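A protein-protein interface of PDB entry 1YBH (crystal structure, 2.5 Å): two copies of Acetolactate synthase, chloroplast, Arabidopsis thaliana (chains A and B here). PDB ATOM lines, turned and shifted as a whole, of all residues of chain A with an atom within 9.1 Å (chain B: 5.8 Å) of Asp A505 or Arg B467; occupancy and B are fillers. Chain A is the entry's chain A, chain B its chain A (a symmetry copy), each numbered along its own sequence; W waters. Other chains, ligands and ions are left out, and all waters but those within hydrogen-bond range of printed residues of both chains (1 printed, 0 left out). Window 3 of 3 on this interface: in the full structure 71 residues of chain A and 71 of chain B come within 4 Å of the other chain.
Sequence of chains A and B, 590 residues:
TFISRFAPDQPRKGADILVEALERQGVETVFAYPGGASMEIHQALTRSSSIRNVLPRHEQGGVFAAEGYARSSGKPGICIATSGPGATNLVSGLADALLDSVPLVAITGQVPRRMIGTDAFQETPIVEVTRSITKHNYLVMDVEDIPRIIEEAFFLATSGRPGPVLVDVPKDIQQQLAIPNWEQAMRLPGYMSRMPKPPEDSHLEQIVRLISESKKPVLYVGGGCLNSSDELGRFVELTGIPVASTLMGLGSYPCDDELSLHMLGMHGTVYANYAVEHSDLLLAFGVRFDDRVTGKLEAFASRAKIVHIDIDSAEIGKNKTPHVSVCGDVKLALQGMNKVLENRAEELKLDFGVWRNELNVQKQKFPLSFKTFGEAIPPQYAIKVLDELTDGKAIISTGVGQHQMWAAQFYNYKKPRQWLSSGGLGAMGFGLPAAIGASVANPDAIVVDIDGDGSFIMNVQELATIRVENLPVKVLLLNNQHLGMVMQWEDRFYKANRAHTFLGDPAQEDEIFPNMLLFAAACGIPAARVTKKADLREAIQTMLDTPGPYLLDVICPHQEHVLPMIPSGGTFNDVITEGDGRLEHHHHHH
No position is printed for both chains.
Printed residues of chain A within 4 Å of Arg B467: Asp A505 (3.9 Å) and Phe A513 (3.8 Å).
Printed residues of chain A within 4 Å of Ala B464: Phe A513 and Pro A514.
Printed residues of chain A within 4 Å of Val B468: Gly A504 (3.6 Å), Asp A505 (3.99 Å), Pro A506 (3.6 Å) and Phe A513 (3.5 Å).
Of the printed residues of chain B, Gly A504 touches Val B468.
The nearest printed residue of chain B that does not touch Asp A505 is Asn B470 (5.0 Å).
The nearest printed residue of chain B that does not touch Phe A513 is Gly B524 (4.3 Å).
Water W1 lies within hydrogen-bond range of OD1 of Asp A505 (2.6 Å), ND2 of Asn B470 (2.8 Å) and O of Val B468 (2.9 Å).
Among the printed residues, merely in contact across the chains: Gly A504 with Val B468 (3.6 Å), Asp A505 with Arg B467 (3.9 Å), Asp A505 with Val B468 (3.99 Å), Pro A506 with Val B468 (3.6 Å), Phe A513 with Ala B464 (3.9 Å), Phe A513 with Arg B467 (3.8 Å), Phe A513 with Val B468 (3.5 Å), Phe A513 with Cys B523 (3.5 Å) and Pro A514 with Ala B464 (3.97 Å).
N of Ala B464 is in hydrogen-bond range of SG of Cys B523 (3.5 Å).
The side-chain carboxylate of Asp A505 is in hydrogen-bond range of the side-chain amide nitrogen of Gln A508 (3.2 Å).
The side-chain amide nitrogen (NE2) of Gln A481 sits close to the backbone NH (N) of Phe A513, at 2.8 Å.
The backbone carbonyl oxygen of Gly B524 is in hydrogen-bond range of the guanidinium group of Arg B467 (3.3 Å).
The guanidinium group (NH1) of Arg B467 is in hydrogen-bond range of the side-chain amide oxygen (OD1) of Asn B470, at 2.7 Å.
The side-chain carboxylate (OD1) of Asp A505 is in hydrogen-bond range of the backbone NH (N) of Ala A507 (2.9 Å).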
ATOM      1  N   ASP A 453      27.110   0.667 -15.498  1.00  0.00           N
ATOM      2  CA  ASP A 453      26.668  -0.112 -16.650  1.00  0.00           C
ATOM      3  C   ASP A 453      26.333  -1.546 -16.273  1.00  0.00           C
ATOM      4  O   ASP A 453      25.487  -2.170 -16.903  1.00  0.00           O
ATOM      5  CB  ASP A 453      27.706  -0.070 -17.791  1.00  0.00           C
ATOM      6  CG  ASP A 453      29.078  -0.574 -17.368  1.00  0.00           C
ATOM      7  OD1 ASP A 453      29.688   0.016 -16.447  1.00  0.00           O
ATOM      8  OD2 ASP A 453      29.550  -1.563 -17.968  1.00  0.00           O
ATOM      9  N   GLN A 481      32.367   0.225 -18.778  1.00  0.00           N
ATOM     10  CA  GLN A 481      32.524  -1.100 -19.375  1.00  0.00           C
ATOM     11  C   GLN A 481      32.996  -2.215 -18.439  1.00  0.00           C
ATOM     12  O   GLN A 481      33.295  -3.321 -18.891  1.00  0.00           O
ATOM     13  CB  GLN A 481      33.492  -1.002 -20.547  1.00  0.00           C
ATOM     14  CG  GLN A 481      33.072  -0.012 -21.611  1.00  0.00           C
ATOM     15  CD  GLN A 481      31.840  -0.467 -22.376  1.00  0.00           C
ATOM     16  OE1 GLN A 481      30.705  -0.246 -21.946  1.00  0.00           O
ATOM     17  NE2 GLN A 481      32.062  -1.117 -23.514  1.00  0.00           N
ATOM     18  N   HIS A 482      33.065  -1.936 -17.142  1.00  0.00           N
ATOM     19  CA  HIS A 482      33.512  -2.943 -16.180  1.00  0.00           C
ATOM     20  C   HIS A 482      32.648  -3.025 -14.923  1.00  0.00           C
ATOM     21  O   HIS A 482      31.717  -2.239 -14.715  1.00  0.00           O
ATOM     22  CB  HIS A 482      34.946  -2.651 -15.714  1.00  0.00           C
ATOM     23  CG  HIS A 482      35.994  -2.881 -16.755  1.00  0.00           C
ATOM     24  ND1 HIS A 482      36.139  -2.069 -17.858  1.00  0.00           N
ATOM     25  CD2 HIS A 482      36.959  -3.828 -16.854  1.00  0.00           C
ATOM     26  CE1 HIS A 482      37.148  -2.505 -18.594  1.00  0.00           C
ATOM     27  NE2 HIS A 482      37.662  -3.572 -18.006  1.00  0.00           N
ATOM     28  N   PHE A 502      34.992  -7.692 -17.166  1.00  0.00           N
ATOM     29  CA  PHE A 502      34.795  -6.839 -18.334  1.00  0.00           C
ATOM     30  C   PHE A 502      33.391  -7.056 -18.887  1.00  0.00           C
ATOM     31  O   PHE A 502      33.026  -8.172 -19.253  1.00  0.00           O
ATOM     32  CB  PHE A 502      35.838  -7.174 -19.407  1.00  0.00           C
ATOM     33  CG  PHE A 502      35.671  -6.396 -20.680  1.00  0.00           C
ATOM     34  CD1 PHE A 502      35.655  -5.006 -20.664  1.00  0.00           C
ATOM     35  CD2 PHE A 502      35.522  -7.055 -21.893  1.00  0.00           C
ATOM     36  CE1 PHE A 502      35.488  -4.282 -21.844  1.00  0.00           C
ATOM     37  CE2 PHE A 502      35.353  -6.338 -23.082  1.00  0.00           C
ATOM     38  CZ  PHE A 502      35.336  -4.948 -23.054  1.00  0.00           C
ATOM     39  N   LEU A 503      32.610  -5.984 -18.958  1.00  0.00           N
ATOM     40  CA  LEU A 503      31.234  -6.072 -19.442  1.00  0.00           C
ATOM     41  C   LEU A 503      31.039  -5.804 -20.933  1.00  0.00           C
ATOM     42  O   LEU A 503      29.935  -5.985 -21.450  1.00  0.00           O
ATOM     43  CB  LEU A 503      30.348  -5.105 -18.653  1.00  0.00           C
ATOM     44  CG  LEU A 503      30.246  -5.356 -17.150  1.00  0.00           C
ATOM     45  CD1 LEU A 503      29.534  -4.196 -16.485  1.00  0.00           C
ATOM     46  CD2 LEU A 503      29.526  -6.664 -16.901  1.00  0.00           C
ATOM     47  N   GLY A 504      32.096  -5.365 -21.617  1.00  0.00           N
ATOM     48  CA  GLY A 504      31.989  -5.076 -23.039  1.00  0.00           C
ATOM     49  C   GLY A 504      32.168  -6.306 -23.904  1.00  0.00           C
ATOM     50  O   GLY A 504      32.117  -7.430 -23.403  1.00  0.00           O
ATOM     51  N   ASP A 505      32.380  -6.100 -25.206  1.00  0.00           N
ATOM     52  CA  ASP A 505      32.570  -7.208 -26.134  1.00  0.00           C
ATOM     53  C   ASP A 505      34.040  -7.366 -26.487  1.00  0.00           C
ATOM     54  O   ASP A 505      34.648  -6.453 -27.038  1.00  0.00           O
ATOM     55  CB  ASP A 505      31.782  -6.983 -27.417  1.00  0.00           C
ATOM     56  CG  ASP A 505      31.783  -8.205 -28.317  1.00  0.00           C
ATOM     57  OD1 ASP A 505      32.605  -9.120 -28.083  1.00  0.00           O
ATOM     58  OD2 ASP A 505      30.963  -8.252 -29.263  1.00  0.00           O
ATOM     59  N   PRO A 506      34.629  -8.529 -26.179  1.00  0.00           N
ATOM     60  CA  PRO A 506      36.037  -8.817 -26.461  1.00  0.00           C
ATOM     61  C   PRO A 506      36.390  -8.771 -27.949  1.00  0.00           C
ATOM     62  O   PRO A 506      37.542  -8.552 -28.304  1.00  0.00           O
ATOM     63  CB  PRO A 506      36.228 -10.208 -25.869  1.00  0.00           C
ATOM     64  CG  PRO A 506      35.241 -10.236 -24.761  1.00  0.00           C
ATOM     65  CD  PRO A 506      34.030  -9.625 -25.404  1.00  0.00           C
ATOM     66  N   ALA A 507      35.401  -8.986 -28.807  1.00  0.00           N
ATOM     67  CA  ALA A 507      35.617  -8.961 -30.249  1.00  0.00           C
ATOM     68  C   ALA A 507      35.814  -7.533 -30.773  1.00  0.00           C
ATOM     69  O   ALA A 507      36.422  -7.332 -31.823  1.00  0.00           O
ATOM     70  CB  ALA A 507      34.442  -9.618 -30.963  1.00  0.00           C
ATOM     71  N   GLN A 508      35.286  -6.553 -30.044  1.00  0.00           N
ATOM     72  CA  GLN A 508      35.404  -5.142 -30.413  1.00  0.00           C
ATOM     73  C   GLN A 508      35.742  -4.379 -29.138  1.00  0.00           C
ATOM     74  O   GLN A 508      35.033  -3.446 -28.767  1.00  0.00           O
ATOM     75  CB  GLN A 508      34.078  -4.619 -30.957  1.00  0.00           C
ATOM     76  CG  GLN A 508      33.241  -5.657 -31.660  1.00  0.00           C
ATOM     77  CD  GLN A 508      31.843  -5.151 -31.965  1.00  0.00           C
ATOM     78  OE1 GLN A 508      31.653  -4.283 -32.826  1.00  0.00           O
ATOM     79  NE2 GLN A 508      30.850  -5.684 -31.247  1.00  0.00           N
ATOM     80  N   GLU A 509      36.823  -4.788 -28.475  1.00  0.00           N
ATOM     81  CA  GLU A 509      37.268  -4.192 -27.213  1.00  0.00           C
ATOM     82  C   GLU A 509      37.176  -2.666 -27.091  1.00  0.00           C
ATOM     83  O   GLU A 509      37.138  -2.137 -25.978  1.00  0.00           O
ATOM     84  CB  GLU A 509      38.699  -4.650 -26.906  1.00  0.00           C
ATOM     85  N   ASP A 510      37.126  -1.957 -28.215  1.00  0.00           N
ATOM     86  CA  ASP A 510      37.063  -0.499 -28.175  1.00  0.00           C
ATOM     87  C   ASP A 510      35.678   0.110 -28.354  1.00  0.00           C
ATOM     88  O   ASP A 510      35.494   1.310 -28.154  1.00  0.00           O
ATOM     89  CB  ASP A 510      38.020   0.089 -29.211  1.00  0.00           C
ATOM     90  CG  ASP A 510      39.473  -0.255 -28.919  1.00  0.00           C
ATOM     91  OD1 ASP A 510      39.933   0.005 -27.783  1.00  0.00           O
ATOM     92  OD2 ASP A 510      40.153  -0.787 -29.827  1.00  0.00           O
ATOM     93  N   GLU A 511      34.705  -0.709 -28.732  1.00  0.00           N
ATOM     94  CA  GLU A 511      33.343  -0.228 -28.918  1.00  0.00           C
ATOM     95  C   GLU A 511      32.560  -0.307 -27.610  1.00  0.00           C
ATOM     96  O   GLU A 511      32.598  -1.325 -26.917  1.00  0.00           O
ATOM     97  CB  GLU A 511      32.635  -1.068 -29.982  1.00  0.00           C
ATOM     98  CG  GLU A 511      33.214  -0.908 -31.364  1.00  0.00           C
ATOM     99  CD  GLU A 511      32.945   0.468 -31.945  1.00  0.00           C
ATOM    100  OE1 GLU A 511      31.793   0.728 -32.357  1.00  0.00           O
ATOM    101  OE2 GLU A 511      33.885   1.292 -31.980  1.00  0.00           O
ATOM    102  N   ILE A 512      31.859   0.769 -27.266  1.00  0.00           N
ATOM    103  CA  ILE A 512      31.053   0.789 -26.050  1.00  0.00           C
ATOM    104  C   ILE A 512      29.967  -0.270 -26.226  1.00  0.00           C
ATOM    105  O   ILE A 512      29.154  -0.178 -27.148  1.00  0.00           O
ATOM    106  CB  ILE A 512      30.387   2.167 -25.849  1.00  0.00           C
ATOM    107  CG1 ILE A 512      31.460   3.242 -25.675  1.00  0.00           C
ATOM    108  CG2 ILE A 512      29.466   2.136 -24.644  1.00  0.00           C
ATOM    109  CD1 ILE A 512      32.408   2.993 -24.515  1.00  0.00           C
ATOM    110  N   PHE A 513      29.962  -1.278 -25.358  1.00  0.00           N
ATOM    111  CA  PHE A 513      28.975  -2.350 -25.450  1.00  0.00           C
ATOM    112  C   PHE A 513      28.368  -2.705 -24.101  1.00  0.00           C
ATOM    113  O   PHE A 513      29.085  -2.890 -23.124  1.00  0.00           O
ATOM    114  CB  PHE A 513      29.613  -3.606 -26.040  1.00  0.00           C
ATOM    115  CG  PHE A 513      28.663  -4.751 -26.172  1.00  0.00           C
ATOM    116  CD1 PHE A 513      27.882  -4.892 -27.310  1.00  0.00           C
ATOM    117  CD2 PHE A 513      28.513  -5.666 -25.135  1.00  0.00           C
ATOM    118  CE1 PHE A 513      26.954  -5.930 -27.420  1.00  0.00           C
ATOM    119  CE2 PHE A 513      27.588  -6.709 -25.227  1.00  0.00           C
ATOM    120  CZ  PHE A 513      26.806  -6.840 -26.374  1.00  0.00           C
ATOM    121  N   PRO A 514      27.032  -2.822 -24.034  1.00  0.00           N
ATOM    122  CA  PRO A 514      26.098  -2.635 -25.150  1.00  0.00           C
ATOM    123  C   PRO A 514      25.861  -1.156 -25.401  1.00  0.00           C
ATOM    124  O   PRO A 514      26.453  -0.302 -24.743  1.00  0.00           O
ATOM    125  CB  PRO A 514      24.816  -3.316 -24.657  1.00  0.00           C
ATOM    126  CG  PRO A 514      25.287  -4.259 -23.608  1.00  0.00           C
ATOM    127  CD  PRO A 514      26.342  -3.456 -22.901  1.00  0.00           C
ATOM    128  N   GLU B 462      20.172 -10.609 -20.954  1.00  0.00           N
ATOM    129  CA  GLU B 462      21.010 -11.710 -21.382  1.00  0.00           C
ATOM    130  C   GLU B 462      21.352 -11.652 -22.873  1.00  0.00           C
ATOM    131  O   GLU B 462      22.166 -12.440 -23.357  1.00  0.00           O
ATOM    132  CB  GLU B 462      20.358 -13.046 -21.022  1.00  0.00           C
ATOM    133  CG  GLU B 462      20.222 -13.272 -19.512  1.00  0.00           C
ATOM    134  CD  GLU B 462      21.498 -12.934 -18.722  1.00  0.00           C
ATOM    135  OE1 GLU B 462      22.611 -13.290 -19.174  1.00  0.00           O
ATOM    136  OE2 GLU B 462      21.385 -12.319 -17.639  1.00  0.00           O
ATOM    137  N   LEU B 463      20.736 -10.724 -23.604  1.00  0.00           N
ATOM    138  CA  LEU B 463      21.033 -10.587 -25.027  1.00  0.00           C
ATOM    139  C   LEU B 463      22.505 -10.215 -25.130  1.00  0.00           C
ATOM    140  O   LEU B 463      23.198 -10.628 -26.059  1.00  0.00           O
ATOM    141  CB  LEU B 463      20.178  -9.496 -25.674  1.00  0.00           C
ATOM    142  CG  LEU B 463      18.687  -9.792 -25.818  1.00  0.00           C
ATOM    143  CD1 LEU B 463      17.963  -8.537 -26.289  1.00  0.00           C
ATOM    144  CD2 LEU B 463      18.483 -10.956 -26.790  1.00  0.00           C
ATOM    145  N   ALA B 464      22.976  -9.436 -24.158  1.00  0.00           N
ATOM    146  CA  ALA B 464      24.368  -9.022 -24.111  1.00  0.00           C
ATOM    147  C   ALA B 464      25.259 -10.257 -24.003  1.00  0.00           C
ATOM    148  O   ALA B 464      26.294 -10.347 -24.660  1.00  0.00           O
ATOM    149  CB  ALA B 464      24.600  -8.108 -22.915  1.00  0.00           C
ATOM    150  N   THR B 465      24.849 -11.203 -23.161  1.00  0.00           N
ATOM    151  CA  THR B 465      25.588 -12.447 -22.955  1.00  0.00           C
ATOM    152  C   THR B 465      25.703 -13.221 -24.268  1.00  0.00           C
ATOM    153  O   THR B 465      26.791 -13.663 -24.658  1.00  0.00           O
ATOM    154  CB  THR B 465      24.870 -13.337 -21.920  1.00  0.00           C
ATOM    155  OG1 THR B 465      24.826 -12.659 -20.659  1.00  0.00           O
ATOM    156  CG2 THR B 465      25.590 -14.663 -21.754  1.00  0.00           C
ATOM    157  N   ILE B 466      24.563 -13.387 -24.936  1.00  0.00           N
ATOM    158  CA  ILE B 466      24.490 -14.096 -26.203  1.00  0.00           C
ATOM    159  C   ILE B 466      25.477 -13.535 -27.226  1.00  0.00           C
ATOM    160  O   ILE B 466      26.205 -14.286 -27.872  1.00  0.00           O
ATOM    161  CB  ILE B 466      23.059 -14.029 -26.784  1.00  0.00           C
ATOM    162  CG1 ILE B 466      22.123 -14.892 -25.936  1.00  0.00           C
ATOM    163  CG2 ILE B 466      23.052 -14.489 -28.240  1.00  0.00           C
ATOM    164  CD1 ILE B 466      20.667 -14.755 -26.298  1.00  0.00           C
ATOM    165  N   ARG B 467      25.509 -12.214 -27.367  1.00  0.00           N
ATOM    166  CA  ARG B 467      26.412 -11.591 -28.323  1.00  0.00           C
ATOM    167  C   ARG B 467      27.870 -11.843 -27.972  1.00  0.00           C
ATOM    168  O   ARG B 467      28.637 -12.369 -28.785  1.00  0.00           O
ATOM    169  CB  ARG B 467      26.149 -10.081 -28.406  1.00  0.00           C
ATOM    170  CG  ARG B 467      27.205  -9.294 -29.195  1.00  0.00           C
ATOM    171  CD  ARG B 467      27.727 -10.080 -30.405  1.00  0.00           C
ATOM    172  NE  ARG B 467      26.753 -10.207 -31.481  1.00  0.00           N
ATOM    173  CZ  ARG B 467      26.832 -11.108 -32.459  1.00  0.00           C
ATOM    174  NH1 ARG B 467      27.835 -11.975 -32.501  1.00  0.00           N
ATOM    175  NH2 ARG B 467      25.916 -11.126 -33.415  1.00  0.00           N
ATOM    176  N   VAL B 468      28.245 -11.464 -26.758  1.00  0.00           N
ATOM    177  CA  VAL B 468      29.607 -11.626 -26.287  1.00  0.00           C
ATOM    178  C   VAL B 468      30.106 -13.069 -26.345  1.00  0.00           C
ATOM    179  O   VAL B 468      31.265 -13.299 -26.680  1.00  0.00           O
ATOM    180  CB  VAL B 468      29.746 -11.071 -24.856  1.00  0.00           C
ATOM    181  CG1 VAL B 468      31.090 -11.444 -24.269  1.00  0.00           C
ATOM    182  CG2 VAL B 468      29.601  -9.559 -24.890  1.00  0.00           C
ATOM    183  N   GLU B 469      29.253 -14.037 -26.029  1.00  0.00           N
ATOM    184  CA  GLU B 469      29.674 -15.439 -26.077  1.00  0.00           C
ATOM    185  C   GLU B 469      29.508 -15.985 -27.496  1.00  0.00           C
ATOM    186  O   GLU B 469      29.774 -17.165 -27.762  1.00  0.00           O
ATOM    187  CB  GLU B 469      28.845 -16.294 -25.110  1.00  0.00           C
ATOM    188  CG  GLU B 469      28.868 -15.851 -23.649  1.00  0.00           C
ATOM    189  CD  GLU B 469      30.253 -15.891 -23.024  1.00  0.00           C
ATOM    190  OE1 GLU B 469      31.003 -16.853 -23.282  1.00  0.00           O
ATOM    191  OE2 GLU B 469      30.589 -14.963 -22.257  1.00  0.00           O
ATOM    192  N   ASN B 470      29.057 -15.116 -28.400  1.00  0.00           N
ATOM    193  CA  ASN B 470      28.833 -15.470 -29.794  1.00  0.00           C
ATOM    194  C   ASN B 470      28.104 -16.809 -29.963  1.00  0.00           C
ATOM    195  O   ASN B 470      28.602 -17.738 -30.601  1.00  0.00           O
ATOM    196  CB  ASN B 470      30.172 -15.447 -30.548  1.00  0.00           C
ATOM    197  CG  ASN B 470      30.522 -14.045 -31.055  1.00  0.00           C
ATOM    198  OD1 ASN B 470      29.924 -13.558 -32.016  1.00  0.00           O
ATOM    199  ND2 ASN B 470      31.470 -13.384 -30.399  1.00  0.00           N
ATOM    200  N   LEU B 471      26.904 -16.873 -29.386  1.00  0.00           N
ATOM    201  CA  LEU B 471      26.049 -18.054 -29.423  1.00  0.00           C
ATOM    202  C   LEU B 471      24.944 -17.904 -30.469  1.00  0.00           C
ATOM    203  O   LEU B 471      24.247 -16.891 -30.521  1.00  0.00           O
ATOM    204  CB  LEU B 471      25.412 -18.273 -28.045  1.00  0.00           C
ATOM    205  CG  LEU B 471      26.374 -18.336 -26.855  1.00  0.00           C
ATOM    206  CD1 LEU B 471      25.580 -18.292 -25.554  1.00  0.00           C
ATOM    207  CD2 LEU B 471      27.232 -19.591 -26.942  1.00  0.00           C
ATOM    208  N   CYS B 523      22.533  -4.775 -28.464  1.00  0.00           N
ATOM    209  CA  CYS B 523      23.513  -5.815 -28.199  1.00  0.00           C
ATOM    210  C   CYS B 523      24.080  -6.384 -29.485  1.00  0.00           C
ATOM    211  O   CYS B 523      24.554  -7.518 -29.518  1.00  0.00           O
ATOM    212  CB  CYS B 523      22.886  -6.932 -27.357  1.00  0.00           C
ATOM    213  SG  CYS B 523      22.242  -6.365 -25.743  1.00  0.00           S
ATOM    214  N   GLY B 524      24.018  -5.586 -30.546  1.00  0.00           N
ATOM    215  CA  GLY B 524      24.558  -6.000 -31.830  1.00  0.00           C
ATOM    216  C   GLY B 524      24.024  -7.308 -32.374  1.00  0.00           C
ATOM    217  O   GLY B 524      24.756  -8.089 -32.985  1.00  0.00           O
ATOM    218  N   ILE B 525      22.741  -7.549 -32.156  1.00  0.00           N
ATOM    219  CA  ILE B 525      22.117  -8.769 -32.629  1.00  0.00           C
ATOM    220  C   ILE B 525      21.127  -8.431 -33.737  1.00  0.00           C
ATOM    221  O   ILE B 525      20.188  -7.663 -33.527  1.00  0.00           O
ATOM    222  CB  ILE B 525      21.388  -9.497 -31.469  1.00  0.00           C
ATOM    223  CG1 ILE B 525      22.418  -9.995 -30.451  1.00  0.00           C
ATOM    224  CG2 ILE B 525      20.543 -10.651 -32.006  1.00  0.00           C
ATOM    225  CD1 ILE B 525      21.807 -10.611 -29.196  1.00  0.00           C
ATOM    226  N   PRO B 526      21.341  -8.989 -34.936  1.00  0.00           N
ATOM    227  CA  PRO B 526      20.456  -8.742 -36.071  1.00  0.00           C
ATOM    228  C   PRO B 526      19.021  -9.157 -35.745  1.00  0.00           C
ATOM    229  O   PRO B 526      18.785 -10.217 -35.157  1.00  0.00           O
ATOM    230  CB  PRO B 526      21.081  -9.583 -37.182  1.00  0.00           C
ATOM    231  CG  PRO B 526      21.740 -10.686 -36.441  1.00  0.00           C
ATOM    232  CD  PRO B 526      22.388  -9.953 -35.302  1.00  0.00           C
ATOM    233  N   GLY B 548      24.797 -16.937 -36.521  1.00  0.00           N
ATOM    234  CA  GLY B 548      24.818 -16.281 -35.225  1.00  0.00           C
ATOM    235  C   GLY B 548      23.448 -16.043 -34.611  1.00  0.00           C
ATOM    236  O   GLY B 548      22.450 -16.612 -35.053  1.00  0.00           O
ATOM    237  N   PRO B 549      23.376 -15.185 -33.585  1.00  0.00           N
ATOM    238  CA  PRO B 549      22.132 -14.851 -32.884  1.00  0.00           C
ATOM    239  C   PRO B 549      21.191 -14.100 -33.813  1.00  0.00           C
ATOM    240  O   PRO B 549      21.635 -13.457 -34.763  1.00  0.00           O
ATOM    241  CB  PRO B 549      22.596 -13.946 -31.746  1.00  0.00           C
ATOM    242  CG  PRO B 549      24.105 -14.100 -31.721  1.00  0.00           C
ATOM    243  CD  PRO B 549      24.473 -14.318 -33.139  1.00  0.00           C
HETATM  244  O   HOH W   1      32.761 -11.691 -28.544  1.00  0.00           O
